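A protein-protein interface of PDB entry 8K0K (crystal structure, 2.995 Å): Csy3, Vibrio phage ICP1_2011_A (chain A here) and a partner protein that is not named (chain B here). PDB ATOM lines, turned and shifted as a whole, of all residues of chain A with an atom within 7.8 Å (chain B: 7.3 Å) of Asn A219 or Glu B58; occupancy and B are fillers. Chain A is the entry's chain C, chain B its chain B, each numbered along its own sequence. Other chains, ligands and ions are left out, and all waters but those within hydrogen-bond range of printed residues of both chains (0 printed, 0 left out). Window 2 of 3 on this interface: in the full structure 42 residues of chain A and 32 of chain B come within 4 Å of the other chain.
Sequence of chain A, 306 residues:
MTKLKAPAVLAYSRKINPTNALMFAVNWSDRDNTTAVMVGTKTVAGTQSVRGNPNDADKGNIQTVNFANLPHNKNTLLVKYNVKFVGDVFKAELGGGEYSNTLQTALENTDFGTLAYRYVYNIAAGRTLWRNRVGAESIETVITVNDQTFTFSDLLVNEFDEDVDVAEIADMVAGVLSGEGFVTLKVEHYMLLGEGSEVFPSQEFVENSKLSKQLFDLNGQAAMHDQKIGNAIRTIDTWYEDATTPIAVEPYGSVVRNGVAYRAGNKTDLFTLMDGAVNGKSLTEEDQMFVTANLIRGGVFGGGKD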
ATOM      1  N   LEU A  22       9.158  15.796  16.401  1.00  0.00           N
ATOM      2  CA  LEU A  22       8.140  16.093  15.405  1.00  0.00           C
ATOM      3  C   LEU A  22       6.758  15.860  15.998  1.00  0.00           C
ATOM      4  O   LEU A  22       6.563  14.950  16.811  1.00  0.00           O
ATOM      5  CB  LEU A  22       8.336  15.241  14.155  1.00  0.00           C
ATOM      6  CG  LEU A  22       9.541  15.652  13.312  1.00  0.00           C
ATOM      7  CD1 LEU A  22       9.586  14.856  12.022  1.00  0.00           C
ATOM      8  CD2 LEU A  22       9.499  17.138  13.024  1.00  0.00           C
ATOM      9  N   ALA A  36       0.526  15.191  10.040  1.00  0.00           N
ATOM     10  CA  ALA A  36       1.438  16.177  10.600  1.00  0.00           C
ATOM     11  C   ALA A  36       0.689  17.437  11.017  1.00  0.00           C
ATOM     12  O   ALA A  36      -0.250  17.876  10.347  1.00  0.00           O
ATOM     13  CB  ALA A  36       2.531  16.522   9.588  1.00  0.00           C
ATOM     14  N   VAL A  37       1.107  18.013  12.139  1.00  0.00           N
ATOM     15  CA  VAL A  37       0.559  19.274  12.623  1.00  0.00           C
ATOM     16  C   VAL A  37       1.356  20.408  11.991  1.00  0.00           C
ATOM     17  O   VAL A  37       2.560  20.545  12.239  1.00  0.00           O
ATOM     18  CB  VAL A  37       0.605  19.349  14.156  1.00  0.00           C
ATOM     19  CG1 VAL A  37       0.111  20.701  14.642  1.00  0.00           C
ATOM     20  CG2 VAL A  37      -0.219  18.229  14.760  1.00  0.00           C
ATOM     21  N   MET A  38       0.695  21.217  11.170  1.00  0.00           N
ATOM     22  CA  MET A  38       1.369  22.266  10.421  1.00  0.00           C
ATOM     23  C   MET A  38       1.258  23.602  11.143  1.00  0.00           C
ATOM     24  O   MET A  38       0.253  23.895  11.796  1.00  0.00           O
ATOM     25  CB  MET A  38       0.794  22.384   9.008  1.00  0.00           C
ATOM     26  CG  MET A  38       0.919  21.105   8.194  1.00  0.00           C
ATOM     27  SD  MET A  38       2.596  20.427   8.141  1.00  0.00           S
ATOM     28  CE  MET A  38       3.254  21.227   6.677  1.00  0.00           C
ATOM     29  N   VAL A  39       2.309  24.407  11.028  1.00  0.00           N
ATOM     30  CA  VAL A  39       2.327  25.740  11.617  1.00  0.00           C
ATOM     31  C   VAL A  39       1.604  26.702  10.683  1.00  0.00           C
ATOM     32  O   VAL A  39       1.908  26.765   9.486  1.00  0.00           O
ATOM     33  CB  VAL A  39       3.768  26.203  11.873  1.00  0.00           C
ATOM     34  CG1 VAL A  39       3.786  27.653  12.326  1.00  0.00           C
ATOM     35  CG2 VAL A  39       4.424  25.318  12.908  1.00  0.00           C
ATOM     36  N   GLN A 214       7.130  33.359  16.545  1.00  0.00           N
ATOM     37  CA  GLN A 214       7.411  32.386  15.501  1.00  0.00           C
ATOM     38  C   GLN A 214       7.625  31.011  16.118  1.00  0.00           C
ATOM     39  O   GLN A 214       8.456  30.853  17.019  1.00  0.00           O
ATOM     40  CB  GLN A 214       8.634  32.788  14.683  1.00  0.00           C
ATOM     41  CG  GLN A 214       8.762  31.967  13.417  1.00  0.00           C
ATOM     42  CD  GLN A 214      10.032  32.237  12.658  1.00  0.00           C
ATOM     43  OE1 GLN A 214      10.437  33.386  12.489  1.00  0.00           O
ATOM     44  NE2 GLN A 214      10.673  31.176  12.194  1.00  0.00           N
ATOM     45  N   LEU A 215       6.884  30.022  15.626  1.00  0.00           N
ATOM     46  CA  LEU A 215       7.020  28.655  16.104  1.00  0.00           C
ATOM     47  C   LEU A 215       7.980  27.878  15.214  1.00  0.00           C
ATOM     48  O   LEU A 215       7.980  28.037  13.990  1.00  0.00           O
ATOM     49  CB  LEU A 215       5.659  27.958  16.146  1.00  0.00           C
ATOM     50  CG  LEU A 215       4.579  28.622  17.004  1.00  0.00           C
ATOM     51  CD1 LEU A 215       3.333  27.771  17.022  1.00  0.00           C
ATOM     52  CD2 LEU A 215       5.060  28.882  18.419  1.00  0.00           C
ATOM     53  N   PHE A 216       8.800  27.042  15.844  1.00  0.00           N
ATOM     54  CA  PHE A 216       9.775  26.232  15.125  1.00  0.00           C
ATOM     55  C   PHE A 216       9.067  25.274  14.172  1.00  0.00           C
ATOM     56  O   PHE A 216       8.075  24.636  14.535  1.00  0.00           O
ATOM     57  CB  PHE A 216      10.633  25.475  16.144  1.00  0.00           C
ATOM     58  CG  PHE A 216      11.643  24.532  15.542  1.00  0.00           C
ATOM     59  CD1 PHE A 216      12.568  24.973  14.616  1.00  0.00           C
ATOM     60  CD2 PHE A 216      11.696  23.206  15.954  1.00  0.00           C
ATOM     61  CE1 PHE A 216      13.504  24.099  14.083  1.00  0.00           C
ATOM     62  CE2 PHE A 216      12.630  22.331  15.428  1.00  0.00           C
ATOM     63  CZ  PHE A 216      13.534  22.777  14.492  1.00  0.00           C
ATOM     64  N   ASP A 217       9.563  25.191  12.939  1.00  0.00           N
ATOM     65  CA  ASP A 217       8.960  24.329  11.933  1.00  0.00           C
ATOM     66  C   ASP A 217      10.040  23.669  11.090  1.00  0.00           C
ATOM     67  O   ASP A 217      11.092  24.255  10.826  1.00  0.00           O
ATOM     68  CB  ASP A 217       8.014  25.099  11.009  1.00  0.00           C
ATOM     69  CG  ASP A 217       8.758  25.884   9.952  1.00  0.00           C
ATOM     70  OD1 ASP A 217       9.351  26.932  10.294  1.00  0.00           O
ATOM     71  OD2 ASP A 217       8.774  25.433   8.785  1.00  0.00           O
ATOM     72  N   LEU A 218       9.763  22.440  10.664  1.00  0.00           N
ATOM     73  CA  LEU A 218      10.624  21.693   9.753  1.00  0.00           C
ATOM     74  C   LEU A 218       9.774  21.355   8.536  1.00  0.00           C
ATOM     75  O   LEU A 218       8.914  20.471   8.601  1.00  0.00           O
ATOM     76  CB  LEU A 218      11.186  20.447  10.426  1.00  0.00           C
ATOM     77  CG  LEU A 218      12.044  20.734  11.661  1.00  0.00           C
ATOM     78  CD1 LEU A 218      12.302  19.473  12.472  1.00  0.00           C
ATOM     79  CD2 LEU A 218      13.355  21.379  11.257  1.00  0.00           C
ATOM     80  N   ASN A 219      10.010  22.076   7.437  1.00  0.00           N
ATOM     81  CA  ASN A 219       9.179  21.997   6.234  1.00  0.00           C
ATOM     82  C   ASN A 219       7.705  22.206   6.565  1.00  0.00           C
ATOM     83  O   ASN A 219       6.825  21.510   6.057  1.00  0.00           O
ATOM     84  CB  ASN A 219       9.388  20.676   5.495  1.00  0.00           C
ATOM     85  CG  ASN A 219      10.697  20.639   4.733  1.00  0.00           C
ATOM     86  OD1 ASN A 219      11.580  19.835   5.035  1.00  0.00           O
ATOM     87  ND2 ASN A 219      10.829  21.511   3.737  1.00  0.00           N
ATOM     88  N   GLY A 220       7.434  23.176   7.437  1.00  0.00           N
ATOM     89  CA  GLY A 220       6.081  23.556   7.769  1.00  0.00           C
ATOM     90  C   GLY A 220       5.443  22.800   8.918  1.00  0.00           C
ATOM     91  O   GLY A 220       4.356  23.192   9.362  1.00  0.00           O
ATOM     92  N   GLN A 221       6.067  21.735   9.412  1.00  0.00           N
ATOM     93  CA  GLN A 221       5.476  20.934  10.476  1.00  0.00           C
ATOM     94  C   GLN A 221       5.981  21.391  11.836  1.00  0.00           C
ATOM     95  O   GLN A 221       7.175  21.647  12.015  1.00  0.00           O
ATOM     96  CB  GLN A 221       5.788  19.453  10.277  1.00  0.00           C
ATOM     97  CG  GLN A 221       5.491  18.601  11.494  1.00  0.00           C
ATOM     98  CD  GLN A 221       5.737  17.129  11.251  1.00  0.00           C
ATOM     99  OE1 GLN A 221       6.490  16.747  10.350  1.00  0.00           O
ATOM    100  NE2 GLN A 221       5.095  16.286  12.054  1.00  0.00           N
ATOM    101  N   ALA A 222       5.061  21.488  12.792  1.00  0.00           N
ATOM    102  CA  ALA A 222       5.419  21.903  14.143  1.00  0.00           C
ATOM    103  C   ALA A 222       6.442  20.947  14.742  1.00  0.00           C
ATOM    104  O   ALA A 222       6.363  19.730  14.558  1.00  0.00           O
ATOM    105  CB  ALA A 222       4.172  21.963  15.026  1.00  0.00           C
ATOM    106  N   ALA A 223       7.410  21.506  15.462  1.00  0.00           N
ATOM    107  CA  ALA A 223       8.488  20.708  16.021  1.00  0.00           C
ATOM    108  C   ALA A 223       8.983  21.364  17.300  1.00  0.00           C
ATOM    109  O   ALA A 223       8.575  22.473  17.657  1.00  0.00           O
ATOM    110  CB  ALA A 223       9.634  20.534  15.016  1.00  0.00           C
ATOM    111  N   ILE B  15      22.697  21.408  13.255  1.00  0.00           N
ATOM    112  CA  ILE B  15      23.942  21.743  12.573  1.00  0.00           C
ATOM    113  C   ILE B  15      24.399  23.148  12.948  1.00  0.00           C
ATOM    114  O   ILE B  15      23.594  24.086  13.018  1.00  0.00           O
ATOM    115  CB  ILE B  15      23.740  21.631  11.053  1.00  0.00           C
ATOM    116  CG1 ILE B  15      23.258  20.237  10.669  1.00  0.00           C
ATOM    117  CG2 ILE B  15      25.007  21.983  10.311  1.00  0.00           C
ATOM    118  CD1 ILE B  15      22.859  20.126   9.213  1.00  0.00           C
ATOM    119  N   ALA B  17      25.434  25.991  11.482  1.00  0.00           N
ATOM    120  CA  ALA B  17      25.291  26.430  10.098  1.00  0.00           C
ATOM    121  C   ALA B  17      26.221  27.572   9.708  1.00  0.00           C
ATOM    122  O   ALA B  17      26.262  27.929   8.525  1.00  0.00           O
ATOM    123  CB  ALA B  17      23.843  26.849   9.832  1.00  0.00           C
ATOM    124  N   VAL B  55      19.294  16.752   0.730  1.00  0.00           N
ATOM    125  CA  VAL B  55      17.935  16.318   0.429  1.00  0.00           C
ATOM    126  C   VAL B  55      16.916  17.284   1.015  1.00  0.00           C
ATOM    127  O   VAL B  55      15.980  17.708   0.334  1.00  0.00           O
ATOM    128  CB  VAL B  55      17.702  14.878   0.939  1.00  0.00           C
ATOM    129  CG1 VAL B  55      16.375  14.342   0.437  1.00  0.00           C
ATOM    130  CG2 VAL B  55      18.847  13.969   0.516  1.00  0.00           C
ATOM    131  N   LYS B  56      17.093  17.653   2.280  1.00  0.00           N
ATOM    132  CA  LYS B  56      16.305  18.715   2.889  1.00  0.00           C
ATOM    133  C   LYS B  56      17.250  19.603   3.685  1.00  0.00           C
ATOM    134  O   LYS B  56      18.288  19.142   4.161  1.00  0.00           O
ATOM    135  CB  LYS B  56      15.193  18.156   3.798  1.00  0.00           C
ATOM    136  CG  LYS B  56      14.100  17.368   3.078  1.00  0.00           C
ATOM    137  CD  LYS B  56      13.133  18.290   2.345  1.00  0.00           C
ATOM    138  CE  LYS B  56      11.961  17.519   1.742  1.00  0.00           C
ATOM    139  NZ  LYS B  56      10.972  18.418   1.072  1.00  0.00           N
ATOM    140  N   PHE B  57      16.896  20.878   3.826  1.00  0.00           N
ATOM    141  CA  PHE B  57      17.731  21.765   4.625  1.00  0.00           C
ATOM    142  C   PHE B  57      16.945  23.009   5.003  1.00  0.00           C
ATOM    143  O   PHE B  57      16.203  23.556   4.186  1.00  0.00           O
ATOM    144  CB  PHE B  57      19.012  22.166   3.886  1.00  0.00           C
ATOM    145  CG  PHE B  57      20.094  22.680   4.792  1.00  0.00           C
ATOM    146  CD1 PHE B  57      20.097  23.996   5.216  1.00  0.00           C
ATOM    147  CD2 PHE B  57      21.105  21.842   5.227  1.00  0.00           C
ATOM    148  CE1 PHE B  57      21.092  24.467   6.056  1.00  0.00           C
ATOM    149  CE2 PHE B  57      22.102  22.307   6.066  1.00  0.00           C
ATOM    150  CZ  PHE B  57      22.096  23.620   6.479  1.00  0.00           C
ATOM    151  N   GLU B  58      17.137  23.457   6.240  1.00  0.00           N
ATOM    152  CA  GLU B  58      16.462  24.652   6.728  1.00  0.00           C
ATOM    153  C   GLU B  58      17.295  25.256   7.845  1.00  0.00           C
ATOM    154  O   GLU B  58      17.602  24.577   8.828  1.00  0.00           O
ATOM    155  CB  GLU B  58      15.057  24.312   7.220  1.00  0.00           C
ATOM    156  CG  GLU B  58      14.159  25.510   7.428  1.00  0.00           C
ATOM    157  CD  GLU B  58      12.728  25.104   7.727  1.00  0.00           C
ATOM    158  OE1 GLU B  58      12.447  23.886   7.722  1.00  0.00           O
ATOM    159  OE2 GLU B  58      11.888  25.998   7.966  1.00  0.00           O
ATOM    160  N   VAL B  59      17.676  26.519   7.683  1.00  0.00           N
ATOM    161  CA  VAL B  59      18.286  27.276   8.766  1.00  0.00           C
ATOM    162  C   VAL B  59      17.186  27.751   9.702  1.00  0.00           C
ATOM    163  O   VAL B  59      16.128  28.217   9.258  1.00  0.00           O
ATOM    164  CB  VAL B  59      19.096  28.461   8.213  1.00  0.00           C
ATOM    165  CG1 VAL B  59      19.859  29.145   9.337  1.00  0.00           C
ATOM    166  CG2 VAL B  59      20.032  28.000   7.108  1.00  0.00           C
ATOM    167  N   ARG B  60      17.418  27.628  11.004  1.00  0.00           N
ATOM    168  CA  ARG B  60      16.424  28.078  11.966  1.00  0.00           C
ATOM    169  C   ARG B  60      16.349  29.599  11.977  1.00  0.00           C
ATOM    170  O   ARG B  60      17.369  30.293  11.914  1.00  0.00           O
ATOM    171  CB  ARG B  60      16.751  27.554  13.361  1.00  0.00           C
ATOM    172  CG  ARG B  60      16.769  26.040  13.464  1.00  0.00           C
ATOM    173  CD  ARG B  60      16.953  25.612  14.905  1.00  0.00           C
ATOM    174  NE  ARG B  60      17.118  24.171  15.041  1.00  0.00           N
ATOM    175  CZ  ARG B  60      17.402  23.566  16.188  1.00  0.00           C
ATOM    176  NH1 ARG B  60      17.553  24.286  17.296  1.00  0.00           N
ATOM    177  NH2 ARG B  60      17.540  22.247  16.228  1.00  0.00           N
ATOM    178  N   GLY B  61      15.128  30.118  12.061  1.00  0.00           N
ATOM    179  CA  GLY B  61      14.883  31.539  12.063  1.00  0.00           C
ATOM    180  C   GLY B  61      13.921  31.904  10.960  1.00  0.00           C
ATOM    181  O   GLY B  61      13.142  31.071  10.487  1.00  0.00           O
ATOM    182  N   LEU B  93      21.924  27.786  13.996  1.00  0.00           N
ATOM    183  CA  LEU B  93      21.775  26.347  13.835  1.00  0.00           C
ATOM    184  C   LEU B  93      20.825  26.040  12.684  1.00  0.00           C
ATOM    185  O   LEU B  93      20.034  26.884  12.256  1.00  0.00           O
ATOM    186  CB  LEU B  93      21.251  25.696  15.119  1.00  0.00           C
ATOM    187  CG  LEU B  93      21.983  25.986  16.428  1.00  0.00           C
ATOM    188  CD1 LEU B  93      21.314  25.250  17.577  1.00  0.00           C
ATOM    189  CD2 LEU B  93      23.444  25.607  16.329  1.00  0.00           C
ATOM    190  N   ALA B  94      20.909  24.812  12.185  1.00  0.00           N
ATOM    191  CA  ALA B  94      20.082  24.389  11.063  1.00  0.00           C
ATOM    192  C   ALA B  94      19.721  22.921  11.223  1.00  0.00           C
ATOM    193  O   ALA B  94      20.218  22.231  12.113  1.00  0.00           O
ATOM    194  CB  ALA B  94      20.784  24.623   9.724  1.00  0.00           C
ATOM    195  N   ASP B  95      18.846  22.446  10.338  1.00  0.00           N
ATOM    196  CA  ASP B  95      18.387  21.063  10.351  1.00  0.00           C
ATOM    197  C   ASP B  95      18.294  20.567   8.918  1.00  0.00           C
ATOM    198  O   ASP B  95      17.824  21.291   8.036  1.00  0.00           O
ATOM    199  CB  ASP B  95      17.022  20.927  11.039  1.00  0.00           C
ATOM    200  CG  ASP B  95      16.955  21.672  12.359  1.00  0.00           C
ATOM    201  OD1 ASP B  95      17.526  21.182  13.358  1.00  0.00           O
ATOM    202  OD2 ASP B  95      16.340  22.763  12.390  1.00  0.00           O
ATOM    203  N   GLY B  96      18.723  19.331   8.683  1.00  0.00           N
ATOM    204  CA  GLY B  96      18.765  18.872   7.309  1.00  0.00           C
ATOM    205  C   GLY B  96      18.749  17.366   7.160  1.00  0.00           C
ATOM    206  O   GLY B  96      18.717  16.611   8.134  1.00  0.00           O
ATOM    207  N   VAL B  97      18.761  16.954   5.893  1.00  0.00           N
ATOM    208  CA  VAL B  97      18.781  15.561   5.457  1.00  0.00           C
ATOM    209  C   VAL B  97      19.727  15.477   4.267  1.00  0.00           C
ATOM    210  O   VAL B  97      19.479  16.113   3.233  1.00  0.00           O
ATOM    211  CB  VAL B  97      17.385  15.050   5.058  1.00  0.00           C
ATOM    212  CG1 VAL B  97      17.480  13.636   4.511  1.00  0.00           C
ATOM    213  CG2 VAL B  97      16.428  15.106   6.238  1.00  0.00           C
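The backbone NH of Asn A219 sits at hydrogen-bond distance from the side-chain carboxylate of Glu B58 (3.0 Å). O of Gly B61 lies within hydrogen-bond range of NE2 of Gln A214 (3.0 Å). OD2 of Asp A217 lies close to OE2 of Glu B58.
O of Lys B56 is in hydrogen-bond range of N of Val B97 (2.8 Å). O of Glu B58 sits at hydrogen-bond distance from N of Asp B95, at 2.9 Å. N of Arg B60 sits at hydrogen-bond distance from O of Leu B93, 3.0 Å away. NH2 of Arg B60 lies within salt-bridge range of OD1 of Asp B95 (3.1 Å). The backbone NH (N) of Ala A223 is in hydrogen-bond range of the backbone carbonyl oxygen (O) of Phe A216, 3.3 Å away. The side-chain carboxylate (OD2) of Asp A217 sits at hydrogen-bond distance from the backbone NH (N) of Gly A220 (3.0 Å).
Among the printed residues, merely in contact across the chains: Asn A219 with Lys B56 (3.5 Å), Leu A218 with Asp B95 (3.5 Å), Leu A218 with Glu B58 (3.5 Å), Phe A216 with Asp B95 (3.5 Å) and Phe A216 with Arg B60 (3.7 Å).
Hydrophobic or aromatic side chains of chain A that line the printed part of chain B: Phe A216 and Leu A218. Among the printed residues, 8 pairs touch across the chains.
Asn A219 touches just these residues of chain B: Lys B56 and Glu B58. Glu B58 touches three residues of chain A. Printed residues of chain B within 4 Å of Asp A217: Glu B58 (3.3 Å). Printed residues of chain A within 4 Å of Asp B95: Phe A216 (3.5 Å) and Leu A218 (3.5 Å). Of the printed residues of chain A, Arg B60 touches Phe A216 (3.7 Å). Val B59 touches none of the printed residues of chain A. Met A38 touches none of the printed residues of chain B. The nearest residue of chain B that does not touch Asn A219 is Phe B57 (5.6 Å).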
